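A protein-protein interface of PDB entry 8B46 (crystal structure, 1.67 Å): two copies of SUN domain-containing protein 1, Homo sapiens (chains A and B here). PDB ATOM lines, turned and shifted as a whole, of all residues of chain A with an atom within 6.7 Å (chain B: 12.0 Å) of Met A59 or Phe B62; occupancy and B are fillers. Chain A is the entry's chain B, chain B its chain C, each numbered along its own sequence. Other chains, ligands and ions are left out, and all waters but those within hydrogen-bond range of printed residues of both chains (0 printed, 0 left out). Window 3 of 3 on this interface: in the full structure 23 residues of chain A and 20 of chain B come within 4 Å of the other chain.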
ATOM      1  N   ALA A  57      -7.607 -23.061  -2.238  1.00  0.00           N
ATOM      2  CA  ALA A  57      -7.865 -21.861  -1.457  1.00  0.00           C
ATOM      3  C   ALA A  57      -6.634 -20.960  -1.412  1.00  0.00           C
ATOM      4  O   ALA A  57      -5.505 -21.388  -1.683  1.00  0.00           O
ATOM      5  CB  ALA A  57      -8.266 -22.245  -0.030  1.00  0.00           C
ATOM      6  N   LEU A  58      -6.869 -19.706  -1.010  1.00  0.00           N
ATOM      7  CA  LEU A  58      -5.816 -18.698  -0.980  1.00  0.00           C
ATOM      8  C   LEU A  58      -4.967 -18.828   0.261  1.00  0.00           C
ATOM      9  O   LEU A  58      -3.754 -18.595   0.202  1.00  0.00           O
ATOM     10  CB  LEU A  58      -6.408 -17.282  -1.031  1.00  0.00           C
ATOM     11  CG  LEU A  58      -7.045 -16.854  -2.359  1.00  0.00           C
ATOM     12  CD1 LEU A  58      -7.811 -15.540  -2.249  1.00  0.00           C
ATOM     13  CD2 LEU A  58      -5.985 -16.794  -3.453  1.00  0.00           C
ATOM     14  N   MET A  59      -5.560 -19.219   1.379  1.00  0.00           N
ATOM     15  CA  MET A  59      -4.742 -19.436   2.557  1.00  0.00           C
ATOM     16  C   MET A  59      -5.327 -20.572   3.377  1.00  0.00           C
ATOM     17  O   MET A  59      -6.267 -21.249   2.956  1.00  0.00           O
ATOM     18  CB  MET A  59      -4.647 -18.149   3.373  1.00  0.00           C
ATOM     19  CG  MET A  59      -5.924 -17.768   4.090  1.00  0.00           C
ATOM     20  SD  MET A  59      -5.976 -15.996   4.402  1.00  0.00           S
ATOM     21  CE  MET A  59      -5.752 -15.429   2.714  1.00  0.00           C
ATOM     22  N   SER A  60      -4.712 -20.824   4.528  1.00  0.00           N
ATOM     23  CA  SER A  60      -5.278 -21.674   5.562  1.00  0.00           C
ATOM     24  C   SER A  60      -5.088 -20.955   6.891  1.00  0.00           C
ATOM     25  O   SER A  60      -4.121 -20.209   7.092  1.00  0.00           O
ATOM     26  CB  SER A  60      -4.660 -23.086   5.600  1.00  0.00           C
ATOM     27  OG  SER A  60      -3.302 -23.054   5.995  1.00  0.00           O
ATOM     28  N   LEU A  61      -6.035 -21.186   7.793  1.00  0.00           N
ATOM     29  CA  LEU A  61      -6.023 -20.616   9.130  1.00  0.00           C
ATOM     30  C   LEU A  61      -6.484 -21.683  10.102  1.00  0.00           C
ATOM     31  O   LEU A  61      -7.565 -22.262   9.926  1.00  0.00           O
ATOM     32  CB  LEU A  61      -6.912 -19.377   9.186  1.00  0.00           C
ATOM     33  CG  LEU A  61      -6.950 -18.531  10.440  1.00  0.00           C
ATOM     34  CD1 LEU A  61      -5.569 -18.083  10.866  1.00  0.00           C
ATOM     35  CD2 LEU A  61      -7.798 -17.343  10.046  1.00  0.00           C
ATOM     36  N   ILE A  64      -7.572 -24.862   8.474  1.00  0.00           N
ATOM     37  CA  ILE A  64      -8.719 -24.829   7.564  1.00  0.00           C
ATOM     38  C   ILE A  64      -8.372 -23.988   6.338  1.00  0.00           C
ATOM     39  O   ILE A  64      -7.996 -22.811   6.492  1.00  0.00           O
ATOM     40  CB  ILE A  64      -9.975 -24.292   8.269  1.00  0.00           C
ATOM     41  CG1 ILE A  64     -10.235 -25.078   9.572  1.00  0.00           C
ATOM     42  CG2 ILE A  64     -11.171 -24.304   7.319  1.00  0.00           C
ATOM     43  CD1 ILE A  64     -10.368 -26.585   9.412  1.00  0.00           C
ATOM     44  N   PRO A  65      -8.487 -24.526   5.118  1.00  0.00           N
ATOM     45  CA  PRO A  65      -8.309 -23.691   3.913  1.00  0.00           C
ATOM     46  C   PRO A  65      -9.432 -22.660   3.764  1.00  0.00           C
ATOM     47  O   PRO A  65     -10.606 -22.988   3.935  1.00  0.00           O
ATOM     48  CB  PRO A  65      -8.339 -24.713   2.768  1.00  0.00           C
ATOM     49  CG  PRO A  65      -8.040 -26.058   3.413  1.00  0.00           C
ATOM     50  CD  PRO A  65      -8.609 -25.969   4.801  1.00  0.00           C
ATOM     51  N   LEU A  66      -9.059 -21.398   3.483  1.00  0.00           N
ATOM     52  CA  LEU A  66      -9.974 -20.267   3.331  1.00  0.00           C
ATOM     53  C   LEU A  66      -9.796 -19.553   1.992  1.00  0.00           C
ATOM     54  O   LEU A  66      -8.660 -19.449   1.465  1.00  0.00           O
ATOM     55  CB  LEU A  66      -9.779 -19.221   4.440  1.00  0.00           C
ATOM     56  CG  LEU A  66      -9.895 -19.708   5.891  1.00  0.00           C
ATOM     57  CD1 LEU A  66      -9.606 -18.522   6.758  1.00  0.00           C
ATOM     58  CD2 LEU A  66     -11.274 -20.316   6.257  1.00  0.00           C
ATOM     59  N   TRP A  67     -10.915 -18.955   1.521  1.00  0.00           N
ATOM     60  CA  TRP A  67     -10.968 -18.135   0.297  1.00  0.00           C
ATOM     61  C   TRP A  67     -10.723 -18.913  -0.987  1.00  0.00           C
ATOM     62  O   TRP A  67      -9.572 -19.064  -1.409  1.00  0.00           O
ATOM     63  CB  TRP A  67      -9.975 -16.977   0.378  1.00  0.00           C
ATOM     64  CG  TRP A  67     -10.079 -16.239   1.651  1.00  0.00           C
ATOM     65  CD1 TRP A  67      -9.181 -16.230   2.718  1.00  0.00           C
ATOM     66  CD2 TRP A  67     -11.134 -15.386   2.013  1.00  0.00           C
ATOM     67  NE1 TRP A  67      -9.653 -15.416   3.731  1.00  0.00           N
ATOM     68  CE2 TRP A  67     -10.843 -14.874   3.315  1.00  0.00           C
ATOM     69  CE3 TRP A  67     -12.322 -15.012   1.379  1.00  0.00           C
ATOM     70  CZ2 TRP A  67     -11.698 -14.003   3.977  1.00  0.00           C
ATOM     71  CZ3 TRP A  67     -13.182 -14.144   2.042  1.00  0.00           C
ATOM     72  CH2 TRP A  67     -12.861 -13.649   3.331  1.00  0.00           C
ATOM     73  N   TYR A  68     -11.760 -19.567  -1.502  1.00  0.00           N
ATOM     74  CA  TYR A  68     -11.659 -20.335  -2.746  1.00  0.00           C
ATOM     75  C   TYR A  68     -12.164 -19.503  -3.921  1.00  0.00           C
ATOM     76  O   TYR A  68     -13.170 -19.845  -4.552  1.00  0.00           O
ATOM     77  CB  TYR A  68     -12.470 -21.621  -2.646  1.00  0.00           C
ATOM     78  CG  TYR A  68     -11.994 -22.644  -1.653  1.00  0.00           C
ATOM     79  CD1 TYR A  68     -12.312 -22.516  -0.311  1.00  0.00           C
ATOM     80  CD2 TYR A  68     -11.283 -23.773  -2.066  1.00  0.00           C
ATOM     81  CE1 TYR A  68     -11.915 -23.493   0.632  1.00  0.00           C
ATOM     82  CE2 TYR A  68     -10.878 -24.756  -1.142  1.00  0.00           C
ATOM     83  CZ  TYR A  68     -11.208 -24.605   0.208  1.00  0.00           C
ATOM     84  OH  TYR A  68     -10.816 -25.539   1.148  1.00  0.00           O
ATOM     85  N   PHE A  69     -11.532 -18.366  -4.205  1.00  0.00           N
ATOM     86  CA  PHE A  69     -12.055 -17.527  -5.282  1.00  0.00           C
ATOM     87  C   PHE A  69     -10.876 -16.863  -5.962  1.00  0.00           C
ATOM     88  O   PHE A  69      -9.748 -16.834  -5.433  1.00  0.00           O
ATOM     89  CB  PHE A  69     -13.065 -16.463  -4.783  1.00  0.00           C
ATOM     90  CG  PHE A  69     -12.408 -15.223  -4.228  1.00  0.00           C
ATOM     91  CD1 PHE A  69     -11.712 -15.266  -3.014  1.00  0.00           C
ATOM     92  CD2 PHE A  69     -12.540 -13.995  -4.891  1.00  0.00           C
ATOM     93  CE1 PHE A  69     -11.081 -14.112  -2.487  1.00  0.00           C
ATOM     94  CE2 PHE A  69     -11.928 -12.837  -4.377  1.00  0.00           C
ATOM     95  CZ  PHE A  69     -11.194 -12.891  -3.161  1.00  0.00           C
ATOM     96  N   SER A  72     -13.284 -10.698  -7.171  1.00  0.00           N
ATOM     97  CA  SER A  72     -14.628 -10.411  -6.726  1.00  0.00           C
ATOM     98  C   SER A  72     -15.374  -9.701  -7.844  1.00  0.00           C
ATOM     99  O   SER A  72     -14.765  -9.195  -8.819  1.00  0.00           O
ATOM    100  CB  SER A  72     -14.583  -9.553  -5.468  1.00  0.00           C
ATOM    101  OG  SER A  72     -14.542  -8.202  -5.822  1.00  0.00           O
ATOM    102  N   LEU B  58     -14.069   2.451  -2.036  1.00  0.00           N
ATOM    103  CA  LEU B  58     -14.225   1.247  -1.221  1.00  0.00           C
ATOM    104  C   LEU B  58     -12.894   0.502  -1.094  1.00  0.00           C
ATOM    105  O   LEU B  58     -12.209   0.248  -2.090  1.00  0.00           O
ATOM    106  CB  LEU B  58     -15.296   0.315  -1.812  1.00  0.00           C
ATOM    107  CG  LEU B  58     -15.528  -1.039  -1.154  1.00  0.00           C
ATOM    108  CD1 LEU B  58     -15.919  -0.933   0.328  1.00  0.00           C
ATOM    109  CD2 LEU B  58     -16.630  -1.760  -1.913  1.00  0.00           C
ATOM    110  N   MET B  59     -12.578   0.064   0.120  1.00  0.00           N
ATOM    111  CA  MET B  59     -11.420  -0.777   0.361  1.00  0.00           C
ATOM    112  C   MET B  59     -11.953  -2.161   0.689  1.00  0.00           C
ATOM    113  O   MET B  59     -12.906  -2.296   1.459  1.00  0.00           O
ATOM    114  CB  MET B  59     -10.591  -0.239   1.529  1.00  0.00           C
ATOM    115  CG  MET B  59      -9.611  -1.251   2.162  1.00  0.00           C
ATOM    116  SD  MET B  59      -8.246  -1.697   1.046  1.00  0.00           S
ATOM    117  CE  MET B  59      -7.551  -0.083   0.571  1.00  0.00           C
ATOM    118  N   SER B  60     -11.320  -3.184   0.119  1.00  0.00           N
ATOM    119  CA  SER B  60     -11.734  -4.562   0.312  1.00  0.00           C
ATOM    120  C   SER B  60     -10.524  -5.420   0.574  1.00  0.00           C
ATOM    121  O   SER B  60      -9.404  -5.081   0.203  1.00  0.00           O
ATOM    122  CB  SER B  60     -12.456  -5.132  -0.919  1.00  0.00           C
ATOM    123  OG  SER B  60     -13.725  -4.559  -1.075  1.00  0.00           O
ATOM    124  N   LEU B  61     -10.767  -6.533   1.236  1.00  0.00           N
ATOM    125  CA  LEU B  61      -9.733  -7.543   1.358  1.00  0.00           C
ATOM    126  C   LEU B  61     -10.382  -8.900   1.142  1.00  0.00           C
ATOM    127  O   LEU B  61     -11.418  -9.194   1.751  1.00  0.00           O
ATOM    128  CB  LEU B  61      -9.001  -7.510   2.706  1.00  0.00           C
ATOM    129  CG  LEU B  61      -7.761  -8.442   2.656  1.00  0.00           C
ATOM    130  CD1 LEU B  61      -6.769  -8.011   1.533  1.00  0.00           C
ATOM    131  CD2 LEU B  61      -7.063  -8.612   4.004  1.00  0.00           C
ATOM    132  N   PHE B  62      -9.781  -9.705   0.257  1.00  0.00           N
ATOM    133  CA  PHE B  62     -10.276 -11.044  -0.089  1.00  0.00           C
ATOM    134  C   PHE B  62     -11.738 -10.958  -0.507  1.00  0.00           C
ATOM    135  O   PHE B  62     -12.588 -11.724  -0.050  1.00  0.00           O
ATOM    136  CB  PHE B  62     -10.091 -12.068   1.065  1.00  0.00           C
ATOM    137  CG  PHE B  62      -8.690 -12.110   1.611  1.00  0.00           C
ATOM    138  CD1 PHE B  62      -7.599 -12.294   0.771  1.00  0.00           C
ATOM    139  CD2 PHE B  62      -8.465 -11.975   2.968  1.00  0.00           C
ATOM    140  CE1 PHE B  62      -6.310 -12.299   1.271  1.00  0.00           C
ATOM    141  CE2 PHE B  62      -7.171 -12.007   3.486  1.00  0.00           C
ATOM    142  CZ  PHE B  62      -6.093 -12.162   2.634  1.00  0.00           C
ATOM    143  N   GLY B  63     -12.058  -9.930  -1.271  1.00  0.00           N
ATOM    144  CA  GLY B  63     -13.407  -9.782  -1.748  1.00  0.00           C
ATOM    145  C   GLY B  63     -14.379  -9.238  -0.731  1.00  0.00           C
ATOM    146  O   GLY B  63     -15.530  -8.956  -1.095  1.00  0.00           O
ATOM    147  N   ILE B  64     -13.944  -9.030   0.508  1.00  0.00           N
ATOM    148  CA  ILE B  64     -14.820  -8.593   1.592  1.00  0.00           C
ATOM    149  C   ILE B  64     -14.728  -7.070   1.660  1.00  0.00           C
ATOM    150  O   ILE B  64     -13.605  -6.538   1.727  1.00  0.00           O
ATOM    151  CB  ILE B  64     -14.420  -9.241   2.931  1.00  0.00           C
ATOM    152  CG1 ILE B  64     -14.307 -10.784   2.817  1.00  0.00           C
ATOM    153  CG2 ILE B  64     -15.385  -8.860   4.088  1.00  0.00           C
ATOM    154  CD1 ILE B  64     -15.560 -11.556   2.311  1.00  0.00           C
ATOM    155  N   PRO B  65     -15.850  -6.336   1.540  1.00  0.00           N
ATOM    156  CA  PRO B  65     -15.796  -4.878   1.715  1.00  0.00           C
ATOM    157  C   PRO B  65     -15.536  -4.536   3.176  1.00  0.00           C
ATOM    158  O   PRO B  65     -16.157  -5.101   4.078  1.00  0.00           O
ATOM    159  CB  PRO B  65     -17.181  -4.398   1.244  1.00  0.00           C
ATOM    160  CG  PRO B  65     -18.045  -5.600   1.172  1.00  0.00           C
ATOM    161  CD  PRO B  65     -17.244  -6.817   1.551  1.00  0.00           C
ATOM    162  N   LEU B  66     -14.621  -3.592   3.408  1.00  0.00           N
ATOM    163  CA  LEU B  66     -14.203  -3.240   4.759  1.00  0.00           C
ATOM    164  C   LEU B  66     -14.644  -1.842   5.179  1.00  0.00           C
ATOM    165  O   LEU B  66     -15.242  -1.685   6.249  1.00  0.00           O
ATOM    166  CB  LEU B  66     -12.672  -3.353   4.870  1.00  0.00           C
ATOM    167  CG  LEU B  66     -12.091  -4.730   4.545  1.00  0.00           C
ATOM    168  CD1 LEU B  66     -10.545  -4.787   4.609  1.00  0.00           C
ATOM    169  CD2 LEU B  66     -12.712  -5.712   5.480  1.00  0.00           C
ATOM    170  N   TRP B  67     -14.381  -0.818   4.362  1.00  0.00           N
ATOM    171  CA  TRP B  67     -14.757   0.565   4.655  1.00  0.00           C
ATOM    172  C   TRP B  67     -14.469   1.465   3.460  1.00  0.00           C
ATOM    173  O   TRP B  67     -13.692   1.118   2.563  1.00  0.00           O
ATOM    174  CB  TRP B  67     -14.041   1.105   5.915  1.00  0.00           C
ATOM    175  CG  TRP B  67     -12.559   1.361   5.707  1.00  0.00           C
ATOM    176  CD1 TRP B  67     -11.979   2.457   5.135  1.00  0.00           C
ATOM    177  CD2 TRP B  67     -11.474   0.514   6.136  1.00  0.00           C
ATOM    178  NE1 TRP B  67     -10.605   2.324   5.133  1.00  0.00           N
ATOM    179  CE2 TRP B  67     -10.269   1.144   5.742  1.00  0.00           C
ATOM    180  CE3 TRP B  67     -11.409  -0.722   6.799  1.00  0.00           C
ATOM    181  CZ2 TRP B  67      -9.013   0.590   5.995  1.00  0.00           C
ATOM    182  CZ3 TRP B  67     -10.157  -1.275   7.053  1.00  0.00           C
ATOM    183  CH2 TRP B  67      -8.974  -0.613   6.650  1.00  0.00           C
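The backbone NH (N) of Leu A58 sits at hydrogen-bond distance from the backbone carbonyl oxygen (O) of Trp A67 (2.8 Å).
O of Met A59 lies within hydrogen-bond range of N of Leu A66.
NE1 of Trp A67 sits close to SD of Met A59 (3.8 Å).
The side-chain hydroxyl (OG) of Ser B60 lies close to the backbone carbonyl oxygen (O) of Ile B64, 3.4 Å away.
Among the printed residues, pairs that only touch across the chains: Trp A67 with Ile B64, Trp A67 with Phe B62, Met A59 with Phe B62, Phe A69 with Phe B62, Phe A69 with Gly B63 and Ser A72 with Gly B63.
No residue of chain B comes within 4 Å of Ala A57.
No residue of chain B comes within 4 Å of Leu A58.
Of chain B, only Phe B62 comes within 4 Å of Met A59.
No residue of chain B comes within 4 Å of Ser A60.
No residue of chain B comes within 4 Å of Leu A61.
No residue of chain B comes within 4 Å of Pro A65.
No residue of chain B comes within 4 Å of Leu A66.
Trp A67 touches just these residues of chain B: Phe B62 (3.3 Å) and Ile B64 (3.3 Å).
Of the printed residues of chain B, Phe A69 touches Phe B62 (3.3 Å) and Gly B63 (3.6 Å).
Of the printed residues of chain B, Ser A72 touches Gly B63 (3.9 Å).
Ser B60 touches none of the printed residues of chain A.
Leu B61 touches none of the printed residues of chain A.
Of the printed residues of chain A, Phe B62 touches Met A59, Trp A67 and Phe A69.
Of the printed residues of chain A, Gly B63 touches Phe A69 and Ser A72.
Of the printed residues of chain A, Ile B64 touches Trp A67.
The nearest residue of chain B that does not touch Met A59 is Leu B61 (7.1 Å).
Of the 10 printed residues of chain B, 3 touch a printed residue of chain A.
Hydrophobic or aromatic side chains of chain B that line the printed part of chain A: Phe B62 and Ile B64.
Along chain B the printed residues that touch a printed residue of chain A span positions 62 to 64.
Along chain A the printed residues that touch a printed residue of chain B span positions 59 to 72.
Among the printed residues, 6 pairs touch across the chains.
Among the printed residues, no Asp or Glu carboxylate lies within 4 Å of a Lys or Arg side-chain nitrogen of the other chain.
Trp A67 touches Ile B64, but with the chains exchanged Ile A64 does not touch Trp B67 (21.7 Å).
8 positions are printed for both chains.
Of the 6 pairs that touch across the chains among the printed residues, none has its exchanged pair printed and touching as well.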
